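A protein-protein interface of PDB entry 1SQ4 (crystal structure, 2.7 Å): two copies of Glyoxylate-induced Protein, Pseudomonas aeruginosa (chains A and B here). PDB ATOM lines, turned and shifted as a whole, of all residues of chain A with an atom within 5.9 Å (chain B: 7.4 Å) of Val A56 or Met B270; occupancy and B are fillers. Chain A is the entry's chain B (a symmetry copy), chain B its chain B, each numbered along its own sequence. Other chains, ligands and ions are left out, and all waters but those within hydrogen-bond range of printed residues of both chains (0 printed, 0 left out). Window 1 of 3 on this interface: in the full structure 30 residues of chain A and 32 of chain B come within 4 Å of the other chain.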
ATOM      1  N   MET A  38     -29.343 -12.302  31.495  1.00  0.00           N
ATOM      2  CA  MET A  38     -28.708 -11.036  31.853  1.00  0.00           C
ATOM      3  C   MET A  38     -27.415 -11.281  32.637  1.00  0.00           C
ATOM      4  O   MET A  38     -27.382 -11.022  33.835  1.00  0.00           O
ATOM      5  CB  MET A  38     -29.648 -10.214  32.743  1.00  0.00           C
ATOM      6  CG  MET A  38     -31.104 -10.162  32.313  1.00  0.00           C
ATOM      7  SD  MET A  38     -31.412  -8.916  30.885  1.00  0.00           S
ATOM      8  CE  MET A  38     -30.700 -10.025  29.439  1.00  0.00           C
ATOM      9  N   VAL A  42     -21.970 -10.861  28.978  1.00  0.00           N
ATOM     10  CA  VAL A  42     -22.774 -10.815  27.778  1.00  0.00           C
ATOM     11  C   VAL A  42     -23.290  -9.401  27.486  1.00  0.00           C
ATOM     12  O   VAL A  42     -24.000  -9.183  26.502  1.00  0.00           O
ATOM     13  CB  VAL A  42     -23.942 -11.830  27.875  1.00  0.00           C
ATOM     14  CG1 VAL A  42     -24.999 -11.347  28.859  1.00  0.00           C
ATOM     15  CG2 VAL A  42     -24.539 -12.057  26.510  1.00  0.00           C
ATOM     16  N   SER A  44     -23.318  -5.343  26.417  1.00  0.00           N
ATOM     17  CA  SER A  44     -22.863  -4.638  25.217  1.00  0.00           C
ATOM     18  C   SER A  44     -22.368  -3.226  25.515  1.00  0.00           C
ATOM     19  O   SER A  44     -22.403  -2.773  26.658  1.00  0.00           O
ATOM     20  CB  SER A  44     -24.001  -4.560  24.202  1.00  0.00           C
ATOM     21  OG  SER A  44     -24.424  -5.855  23.823  1.00  0.00           O
ATOM     22  N   LEU A  46     -21.895   1.021  23.751  1.00  0.00           N
ATOM     23  CA  LEU A  46     -22.146   1.999  22.697  1.00  0.00           C
ATOM     24  C   LEU A  46     -21.092   3.090  22.797  1.00  0.00           C
ATOM     25  O   LEU A  46     -20.617   3.409  23.885  1.00  0.00           O
ATOM     26  CB  LEU A  46     -23.537   2.630  22.839  1.00  0.00           C
ATOM     27  CG  LEU A  46     -24.758   1.803  22.437  1.00  0.00           C
ATOM     28  CD1 LEU A  46     -26.006   2.456  23.006  1.00  0.00           C
ATOM     29  CD2 LEU A  46     -24.847   1.694  20.919  1.00  0.00           C
ATOM     30  N   MET A  54     -24.827  -2.367  29.199  1.00  0.00           N
ATOM     31  CA  MET A  54     -26.230  -2.588  28.913  1.00  0.00           C
ATOM     32  C   MET A  54     -26.478  -3.970  28.348  1.00  0.00           C
ATOM     33  O   MET A  54     -25.557  -4.639  27.874  1.00  0.00           O
ATOM     34  CB  MET A  54     -26.733  -1.544  27.919  1.00  0.00           C
ATOM     35  CG  MET A  54     -25.873  -1.429  26.671  1.00  0.00           C
ATOM     36  SD  MET A  54     -26.746  -0.408  25.303  1.00  0.00           S
ATOM     37  CE  MET A  54     -26.368  -1.483  23.761  1.00  0.00           C
ATOM     38  N   TRP A  55     -27.737  -4.389  28.409  1.00  0.00           N
ATOM     39  CA  TRP A  55     -28.163  -5.685  27.896  1.00  0.00           C
ATOM     40  C   TRP A  55     -29.079  -5.389  26.744  1.00  0.00           C
ATOM     41  O   TRP A  55     -29.983  -4.572  26.871  1.00  0.00           O
ATOM     42  CB  TRP A  55     -28.920  -6.447  28.972  1.00  0.00           C
ATOM     43  CG  TRP A  55     -28.017  -7.020  30.006  1.00  0.00           C
ATOM     44  CD1 TRP A  55     -27.277  -8.171  29.904  1.00  0.00           C
ATOM     45  CD2 TRP A  55     -27.722  -6.465  31.288  1.00  0.00           C
ATOM     46  NE1 TRP A  55     -26.545  -8.365  31.046  1.00  0.00           N
ATOM     47  CE2 TRP A  55     -26.801  -7.337  31.916  1.00  0.00           C
ATOM     48  CE3 TRP A  55     -28.146  -5.319  31.973  1.00  0.00           C
ATOM     49  CZ2 TRP A  55     -26.295  -7.097  33.199  1.00  0.00           C
ATOM     50  CZ3 TRP A  55     -27.637  -5.082  33.253  1.00  0.00           C
ATOM     51  CH2 TRP A  55     -26.726  -5.970  33.847  1.00  0.00           C
ATOM     52  N   VAL A  56     -28.852  -6.038  25.615  1.00  0.00           N
ATOM     53  CA  VAL A  56     -29.691  -5.789  24.461  1.00  0.00           C
ATOM     54  C   VAL A  56     -30.785  -6.827  24.345  1.00  0.00           C
ATOM     55  O   VAL A  56     -30.567  -8.014  24.569  1.00  0.00           O
ATOM     56  CB  VAL A  56     -28.875  -5.793  23.162  1.00  0.00           C
ATOM     57  CG1 VAL A  56     -29.751  -5.378  21.994  1.00  0.00           C
ATOM     58  CG2 VAL A  56     -27.707  -4.859  23.295  1.00  0.00           C
ATOM     59  N   ILE A  57     -31.982  -6.365  24.019  1.00  0.00           N
ATOM     60  CA  ILE A  57     -33.104  -7.263  23.839  1.00  0.00           C
ATOM     61  C   ILE A  57     -33.810  -6.839  22.559  1.00  0.00           C
ATOM     62  O   ILE A  57     -34.705  -5.995  22.562  1.00  0.00           O
ATOM     63  CB  ILE A  57     -34.080  -7.223  25.047  1.00  0.00           C
ATOM     64  CG1 ILE A  57     -35.428  -7.808  24.645  1.00  0.00           C
ATOM     65  CG2 ILE A  57     -34.256  -5.820  25.534  1.00  0.00           C
ATOM     66  CD1 ILE A  57     -35.321  -9.209  24.091  1.00  0.00           C
ATOM     67  N   ALA A  58     -33.367  -7.428  21.457  1.00  0.00           N
ATOM     68  CA  ALA A  58     -33.923  -7.143  20.145  1.00  0.00           C
ATOM     69  C   ALA A  58     -33.902  -8.412  19.307  1.00  0.00           C
ATOM     70  O   ALA A  58     -33.223  -9.376  19.651  1.00  0.00           O
ATOM     71  CB  ALA A  58     -33.119  -6.059  19.470  1.00  0.00           C
ATOM     72  N   ARG A  59     -34.650  -8.406  18.208  1.00  0.00           N
ATOM     73  CA  ARG A  59     -34.728  -9.556  17.311  1.00  0.00           C
ATOM     74  C   ARG A  59     -34.880 -10.863  18.092  1.00  0.00           C
ATOM     75  O   ARG A  59     -34.090 -11.782  17.936  1.00  0.00           O
ATOM     76  CB  ARG A  59     -33.479  -9.617  16.438  1.00  0.00           C
ATOM     77  CG  ARG A  59     -33.266  -8.377  15.612  1.00  0.00           C
ATOM     78  CD  ARG A  59     -32.346  -8.650  14.427  1.00  0.00           C
ATOM     79  NE  ARG A  59     -30.943  -8.864  14.795  1.00  0.00           N
ATOM     80  CZ  ARG A  59     -30.099  -7.890  15.127  1.00  0.00           C
ATOM     81  NH1 ARG A  59     -30.505  -6.627  15.147  1.00  0.00           N
ATOM     82  NH2 ARG A  59     -28.844  -8.176  15.412  1.00  0.00           N
ATOM     83  N   SER A  69     -36.107  -1.626  19.241  1.00  0.00           N
ATOM     84  CA  SER A  69     -34.838  -1.943  19.875  1.00  0.00           C
ATOM     85  C   SER A  69     -35.101  -1.713  21.357  1.00  0.00           C
ATOM     86  O   SER A  69     -35.872  -0.819  21.718  1.00  0.00           O
ATOM     87  CB  SER A  69     -33.751  -0.990  19.386  1.00  0.00           C
ATOM     88  OG  SER A  69     -32.940  -0.542  20.459  1.00  0.00           O
ATOM     89  N   GLN A  70     -34.485  -2.514  22.215  1.00  0.00           N
ATOM     90  CA  GLN A  70     -34.679  -2.337  23.642  1.00  0.00           C
ATOM     91  C   GLN A  70     -33.397  -2.615  24.386  1.00  0.00           C
ATOM     92  O   GLN A  70     -32.816  -3.684  24.216  1.00  0.00           O
ATOM     93  CB  GLN A  70     -35.755  -3.283  24.148  1.00  0.00           C
ATOM     94  CG  GLN A  70     -36.178  -2.993  25.562  1.00  0.00           C
ATOM     95  CD  GLN A  70     -37.002  -4.104  26.147  1.00  0.00           C
ATOM     96  OE1 GLN A  70     -37.608  -4.880  25.418  1.00  0.00           O
ATOM     97  NE2 GLN A  70     -37.042  -4.181  27.471  1.00  0.00           N
ATOM     98  N   TYR A  71     -32.929  -1.665  25.193  1.00  0.00           N
ATOM     99  CA  TYR A  71     -31.708  -1.904  25.977  1.00  0.00           C
ATOM    100  C   TYR A  71     -31.998  -1.677  27.455  1.00  0.00           C
ATOM    101  O   TYR A  71     -32.808  -0.824  27.808  1.00  0.00           O
ATOM    102  CB  TYR A  71     -30.557  -0.957  25.592  1.00  0.00           C
ATOM    103  CG  TYR A  71     -30.274  -0.742  24.114  1.00  0.00           C
ATOM    104  CD1 TYR A  71     -30.308  -1.794  23.200  1.00  0.00           C
ATOM    105  CD2 TYR A  71     -29.923   0.529  23.640  1.00  0.00           C
ATOM    106  CE1 TYR A  71     -30.004  -1.586  21.852  1.00  0.00           C
ATOM    107  CE2 TYR A  71     -29.613   0.742  22.296  1.00  0.00           C
ATOM    108  CZ  TYR A  71     -29.658  -0.316  21.410  1.00  0.00           C
ATOM    109  OH  TYR A  71     -29.354  -0.114  20.089  1.00  0.00           O
ATOM    110  N   ILE A  72     -31.360  -2.453  28.320  1.00  0.00           N
ATOM    111  CA  ILE A  72     -31.530  -2.249  29.753  1.00  0.00           C
ATOM    112  C   ILE A  72     -30.164  -1.702  30.150  1.00  0.00           C
ATOM    113  O   ILE A  72     -29.206  -2.453  30.316  1.00  0.00           O
ATOM    114  CB  ILE A  72     -31.856  -3.563  30.515  1.00  0.00           C
ATOM    115  CG1 ILE A  72     -33.219  -4.097  30.095  1.00  0.00           C
ATOM    116  CG2 ILE A  72     -31.944  -3.294  32.006  1.00  0.00           C
ATOM    117  CD1 ILE A  72     -33.624  -5.344  30.838  1.00  0.00           C
ATOM    118  N   ARG A 142     -36.165   2.273  21.578  1.00  0.00           N
ATOM    119  CA  ARG A 142     -36.122   3.148  20.408  1.00  0.00           C
ATOM    120  C   ARG A 142     -36.845   2.649  19.169  1.00  0.00           C
ATOM    121  O   ARG A 142     -37.228   1.484  19.075  1.00  0.00           O
ATOM    122  CB  ARG A 142     -34.679   3.500  20.048  1.00  0.00           C
ATOM    123  CG  ARG A 142     -33.669   2.469  20.453  1.00  0.00           C
ATOM    124  CD  ARG A 142     -32.377   3.143  20.909  1.00  0.00           C
ATOM    125  NE  ARG A 142     -31.662   3.785  19.802  1.00  0.00           N
ATOM    126  CZ  ARG A 142     -31.311   3.158  18.683  1.00  0.00           C
ATOM    127  NH1 ARG A 142     -31.611   1.873  18.519  1.00  0.00           N
ATOM    128  NH2 ARG A 142     -30.658   3.813  17.737  1.00  0.00           N
ATOM    129  N   GLN B 146     -19.319  -0.512  10.106  1.00  0.00           N
ATOM    130  CA  GLN B 146     -20.302   0.504  10.424  1.00  0.00           C
ATOM    131  C   GLN B 146     -19.602   1.747  10.954  1.00  0.00           C
ATOM    132  O   GLN B 146     -19.160   1.784  12.098  1.00  0.00           O
ATOM    133  CB  GLN B 146     -21.287  -0.051  11.451  1.00  0.00           C
ATOM    134  CG  GLN B 146     -22.474   0.836  11.769  1.00  0.00           C
ATOM    135  CD  GLN B 146     -23.634   0.041  12.348  1.00  0.00           C
ATOM    136  OE1 GLN B 146     -24.643   0.611  12.768  1.00  0.00           O
ATOM    137  NE2 GLN B 146     -23.496  -1.291  12.366  1.00  0.00           N
ATOM    138  N   HIS B 210     -22.187 -13.841  23.866  1.00  0.00           N
ATOM    139  CA  HIS B 210     -22.877 -12.814  23.114  1.00  0.00           C
ATOM    140  C   HIS B 210     -24.363 -13.138  23.194  1.00  0.00           C
ATOM    141  O   HIS B 210     -24.744 -14.309  23.230  1.00  0.00           O
ATOM    142  CB  HIS B 210     -22.397 -12.814  21.660  1.00  0.00           C
ATOM    143  CG  HIS B 210     -22.846 -11.620  20.872  1.00  0.00           C
ATOM    144  ND1 HIS B 210     -22.656 -10.325  21.307  1.00  0.00           N
ATOM    145  CD2 HIS B 210     -23.467 -11.530  19.672  1.00  0.00           C
ATOM    146  CE1 HIS B 210     -23.144  -9.489  20.408  1.00  0.00           C
ATOM    147  NE2 HIS B 210     -23.642 -10.193  19.407  1.00  0.00           N
ATOM    148  N   VAL B 211     -25.189 -12.099  23.242  1.00  0.00           N
ATOM    149  CA  VAL B 211     -26.632 -12.257  23.340  1.00  0.00           C
ATOM    150  C   VAL B 211     -27.270 -12.345  21.947  1.00  0.00           C
ATOM    151  O   VAL B 211     -28.211 -13.108  21.738  1.00  0.00           O
ATOM    152  CB  VAL B 211     -27.239 -11.083  24.199  1.00  0.00           C
ATOM    153  CG1 VAL B 211     -27.024  -9.751  23.504  1.00  0.00           C
ATOM    154  CG2 VAL B 211     -28.698 -11.310  24.470  1.00  0.00           C
ATOM    155  N   MET B 212     -26.747 -11.590  20.986  1.00  0.00           N
ATOM    156  CA  MET B 212     -27.284 -11.625  19.624  1.00  0.00           C
ATOM    157  C   MET B 212     -26.646 -12.761  18.809  1.00  0.00           C
ATOM    158  O   MET B 212     -25.786 -13.489  19.310  1.00  0.00           O
ATOM    159  CB  MET B 212     -27.047 -10.284  18.926  1.00  0.00           C
ATOM    160  CG  MET B 212     -27.754  -9.103  19.586  1.00  0.00           C
ATOM    161  SD  MET B 212     -29.702  -9.264  19.539  1.00  0.00           S
ATOM    162  CE  MET B 212     -30.061  -9.719  21.394  1.00  0.00           C
ATOM    163  N   GLU B 213     -27.053 -12.904  17.553  1.00  0.00           N
ATOM    164  CA  GLU B 213     -26.523 -13.969  16.719  1.00  0.00           C
ATOM    165  C   GLU B 213     -25.011 -13.931  16.486  1.00  0.00           C
ATOM    166  O   GLU B 213     -24.418 -12.868  16.339  1.00  0.00           O
ATOM    167  CB  GLU B 213     -27.265 -14.024  15.367  1.00  0.00           C
ATOM    168  CG  GLU B 213     -27.352 -12.722  14.569  1.00  0.00           C
ATOM    169  CD  GLU B 213     -28.361 -11.734  15.127  1.00  0.00           C
ATOM    170  OE1 GLU B 213     -29.551 -12.092  15.284  1.00  0.00           O
ATOM    171  OE2 GLU B 213     -27.965 -10.588  15.408  1.00  0.00           O
ATOM    172  N   PHE B 245     -30.065 -15.133  21.962  1.00  0.00           N
ATOM    173  CA  PHE B 245     -30.534 -15.570  23.267  1.00  0.00           C
ATOM    174  C   PHE B 245     -30.434 -17.081  23.358  1.00  0.00           C
ATOM    175  O   PHE B 245     -30.651 -17.665  24.413  1.00  0.00           O
ATOM    176  CB  PHE B 245     -31.976 -15.103  23.491  1.00  0.00           C
ATOM    177  CG  PHE B 245     -32.107 -13.622  23.607  1.00  0.00           C
ATOM    178  CD1 PHE B 245     -31.635 -12.961  24.736  1.00  0.00           C
ATOM    179  CD2 PHE B 245     -32.636 -12.875  22.562  1.00  0.00           C
ATOM    180  CE1 PHE B 245     -31.688 -11.571  24.826  1.00  0.00           C
ATOM    181  CE2 PHE B 245     -32.694 -11.481  22.639  1.00  0.00           C
ATOM    182  CZ  PHE B 245     -32.214 -10.829  23.774  1.00  0.00           C
ATOM    183  N   ASP B 265     -20.910  -9.109  16.034  1.00  0.00           N
ATOM    184  CA  ASP B 265     -20.893  -7.665  15.843  1.00  0.00           C
ATOM    185  C   ASP B 265     -21.182  -7.017  17.182  1.00  0.00           C
ATOM    186  O   ASP B 265     -21.961  -7.535  17.983  1.00  0.00           O
ATOM    187  CB  ASP B 265     -21.940  -7.255  14.824  1.00  0.00           C
ATOM    188  CG  ASP B 265     -23.287  -7.810  15.152  1.00  0.00           C
ATOM    189  OD1 ASP B 265     -23.353  -9.012  15.513  1.00  0.00           O
ATOM    190  OD2 ASP B 265     -24.288  -7.062  15.043  1.00  0.00           O
ATOM    191  N   VAL B 266     -20.557  -5.872  17.418  1.00  0.00           N
ATOM    192  CA  VAL B 266     -20.714  -5.189  18.686  1.00  0.00           C
ATOM    193  C   VAL B 266     -20.447  -3.694  18.588  1.00  0.00           C
ATOM    194  O   VAL B 266     -20.178  -3.169  17.505  1.00  0.00           O
ATOM    195  CB  VAL B 266     -19.730  -5.784  19.714  1.00  0.00           C
ATOM    196  CG1 VAL B 266     -20.001  -7.271  19.915  1.00  0.00           C
ATOM    197  CG2 VAL B 266     -18.296  -5.597  19.214  1.00  0.00           C
ATOM    198  N   ASN B 267     -20.515  -3.039  19.748  1.00  0.00           N
ATOM    199  CA  ASN B 267     -20.274  -1.604  19.933  1.00  0.00           C
ATOM    200  C   ASN B 267     -21.070  -0.671  19.048  1.00  0.00           C
ATOM    201  O   ASN B 267     -20.641   0.452  18.771  1.00  0.00           O
ATOM    202  CB  ASN B 267     -18.796  -1.280  19.758  1.00  0.00           C
ATOM    203  CG  ASN B 267     -17.916  -2.084  20.676  1.00  0.00           C
ATOM    204  OD1 ASN B 267     -18.218  -2.254  21.853  1.00  0.00           O
ATOM    205  ND2 ASN B 267     -16.807  -2.570  20.145  1.00  0.00           N
ATOM    206  N   ARG B 268     -22.237  -1.116  18.615  1.00  0.00           N
ATOM    207  CA  ARG B 268     -23.042  -0.283  17.747  1.00  0.00           C
ATOM    208  C   ARG B 268     -24.520  -0.395  18.116  1.00  0.00           C
ATOM    209  O   ARG B 268     -24.898  -1.284  18.869  1.00  0.00           O
ATOM    210  CB  ARG B 268     -22.800  -0.722  16.315  1.00  0.00           C
ATOM    211  CG  ARG B 268     -22.580   0.419  15.359  1.00  0.00           C
ATOM    212  CD  ARG B 268     -21.109   0.621  14.941  1.00  0.00           C
ATOM    213  NE  ARG B 268     -20.207   0.923  16.047  1.00  0.00           N
ATOM    214  CZ  ARG B 268     -18.944   1.321  15.895  1.00  0.00           C
ATOM    215  NH1 ARG B 268     -18.189   1.565  16.956  1.00  0.00           N
ATOM    216  NH2 ARG B 268     -18.431   1.495  14.684  1.00  0.00           N
ATOM    217  N   HIS B 269     -25.353   0.509  17.615  1.00  0.00           N
ATOM    218  CA  HIS B 269     -26.778   0.444  17.919  1.00  0.00           C
ATOM    219  C   HIS B 269     -27.381  -0.717  17.152  1.00  0.00           C
ATOM    220  O   HIS B 269     -26.771  -1.231  16.212  1.00  0.00           O
ATOM    221  CB  HIS B 269     -27.491   1.737  17.503  1.00  0.00           C
ATOM    222  CG  HIS B 269     -27.634   2.734  18.610  1.00  0.00           C
ATOM    223  ND1 HIS B 269     -28.513   2.561  19.657  1.00  0.00           N
ATOM    224  CD2 HIS B 269     -26.966   3.885  18.861  1.00  0.00           C
ATOM    225  CE1 HIS B 269     -28.375   3.562  20.512  1.00  0.00           C
ATOM    226  NE2 HIS B 269     -27.443   4.377  20.052  1.00  0.00           N
ATOM    227  N   MET B 270     -28.577  -1.135  17.547  1.00  0.00           N
ATOM    228  CA  MET B 270     -29.247  -2.226  16.853  1.00  0.00           C
ATOM    229  C   MET B 270     -29.960  -1.670  15.626  1.00  0.00           C
ATOM    230  O   MET B 270     -30.616  -0.632  15.697  1.00  0.00           O
ATOM    231  CB  MET B 270     -30.256  -2.903  17.777  1.00  0.00           C
ATOM    232  CG  MET B 270     -29.627  -3.687  18.917  1.00  0.00           C
ATOM    233  SD  MET B 270     -28.567  -5.144  18.255  1.00  0.00           S
ATOM    234  CE  MET B 270     -26.830  -4.357  18.513  1.00  0.00           C
ATOM    235  N   ARG B 271     -29.834  -2.360  14.497  1.00  0.00           N
ATOM    236  CA  ARG B 271     -30.459  -1.909  13.257  1.00  0.00           C
ATOM    237  C   ARG B 271     -31.976  -1.783  13.363  1.00  0.00           C
ATOM    238  O   ARG B 271     -32.665  -2.731  13.730  1.00  0.00           O
ATOM    239  CB  ARG B 271     -30.089  -2.849  12.102  1.00  0.00           C
ATOM    240  CG  ARG B 271     -30.139  -4.333  12.455  1.00  0.00           C
ATOM    241  CD  ARG B 271     -28.852  -4.810  13.172  1.00  0.00           C
ATOM    242  NE  ARG B 271     -27.712  -4.946  12.256  1.00  0.00           N
ATOM    243  CZ  ARG B 271     -26.516  -5.425  12.603  1.00  0.00           C
ATOM    244  NH1 ARG B 271     -25.542  -5.510  11.701  1.00  0.00           N
ATOM    245  NH2 ARG B 271     -26.296  -5.816  13.855  1.00  0.00           N
ATOM    246  N   LEU B 272     -32.494  -0.605  13.040  1.00  0.00           N
ATOM    247  CA  LEU B 272     -33.932  -0.371  13.102  1.00  0.00           C
ATOM    248  C   LEU B 272     -34.519  -0.216  11.708  1.00  0.00           C
ATOM    249  O   LEU B 272     -33.888   0.344  10.818  1.00  0.00           O
ATOM    250  CB  LEU B 272     -34.230   0.891  13.910  1.00  0.00           C
ATOM    251  CG  LEU B 272     -34.042   0.852  15.426  1.00  0.00           C
ATOM    252  CD1 LEU B 272     -34.082   2.263  15.973  1.00  0.00           C
ATOM    253  CD2 LEU B 272     -35.122  -0.001  16.058  1.00  0.00           C
ATOM    254  N   THR B 273     -35.732  -0.712  11.521  1.00  0.00           N
ATOM    255  CA  THR B 273     -36.389  -0.604  10.230  1.00  0.00           C
ATOM    256  C   THR B 273     -36.560   0.870   9.880  1.00  0.00           C
ATOM    257  O   THR B 273     -37.066   1.652  10.684  1.00  0.00           O
ATOM    258  CB  THR B 273     -37.766  -1.282  10.254  1.00  0.00           C
ATOM    259  OG1 THR B 273     -37.604  -2.673  10.553  1.00  0.00           O
ATOM    260  CG2 THR B 273     -38.456  -1.130   8.913  1.00  0.00           C
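OE2 of Glu B213 is in salt-bridge range of NH2 of Arg A59 (2.6 Å). The side-chain hydroxyl (OH) of Tyr A71 lies within hydrogen-bond range of a ring nitrogen (ND1) of His B269, at 2.8 Å. The guanidinium group of Arg A142 lies close to a ring nitrogen (ND1) of His B269 (3.1 Å). N of Met B270 sits at hydrogen-bond distance from OH of Tyr A71 (2.8 Å). The side-chain sulfur (SD) of Met B212 lies close to the backbone carbonyl oxygen (O) of Ala A58, at 3.5 Å.
The backbone carbonyl oxygen of Gln B146 sits at hydrogen-bond distance from the guanidinium group of Arg B268, 2.7 Å away. A ring nitrogen (NE2) of His B210 sits close to the backbone carbonyl oxygen (O) of Asp B265, 3.5 Å away. N of Phe B245 is in hydrogen-bond range of O of Val B211, 2.8 Å away. The side-chain carboxylate (OD2) of Asp B265 lies within salt-bridge range of the guanidinium group (NH2) of Arg B271 (2.6 Å). The backbone NH (N) of Ile A57 sits at hydrogen-bond distance from the backbone carbonyl oxygen (O) of Gln A70, at 2.8 Å. OH of Tyr A71 lies within hydrogen-bond range of NH1 of Arg A142 (3.4 Å).
Among the printed residues, merely in contact across the chains: Arg A59 with Arg B271 (3.2 Å), Val A42 with Val B211 (3.3 Å), Val A56 with Phe B245 (3.4 Å), Val A42 with His B210 (3.5 Å), Leu A46 with Arg B268 (3.5 Å), Val A56 with Met B270 (3.5 Å), Ile A57 with Phe B245 (3.5 Å), Leu A46 with His B269 (3.5 Å), Arg A142 with Leu B272 (3.6 Å), Val A56 with Met B212 (3.6 Å), Ala A58 with Phe B245 (3.7 Å), Ser A69 with Leu B272 (3.7 Å), Val A56 with Val B211 (3.8 Å), Arg A142 with Met B270 (3.9 Å) and Arg A59 with Met B270 (3.95 Å).
Met B270 touches four residues of chain A. Of the printed residues of chain A, Met B212 touches Val A56 (3.6 Å) and Ala A58 (3.5 Å). Of the printed residues of chain A, Arg B271 touches Arg A59 (3.2 Å). Printed residues of chain B within 4 Å of Val A42: His B210 (3.5 Å) and Val B211 (3.3 Å). Of the printed residues of chain B, Ile A57 touches Phe B245 (3.5 Å). The nearest residue of chain B that does not touch Val A56 is Arg B268 (6.3 Å).
Of the 15 printed residues of chain A, 9 touch a printed residue of chain B. Printed residues of chain A that touch a printed residue of chain B: Val A42, Leu A46, Val A56, Ile A57, Ala A58, Arg A59, Ser A69, Tyr A71 and Arg A142. Hydrophobic or aromatic side chains of chain A within 4 Å of the printed part of chain B: Val A42, Leu A46, Val A56, Ile A57 and Tyr A71. Among the printed residues, 20 pairs touch across the chains.
No position is printed for both chains. Of the 20 pairs that touch across the chains among the printed residues, none has its exchanged pair printed and touching as well.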
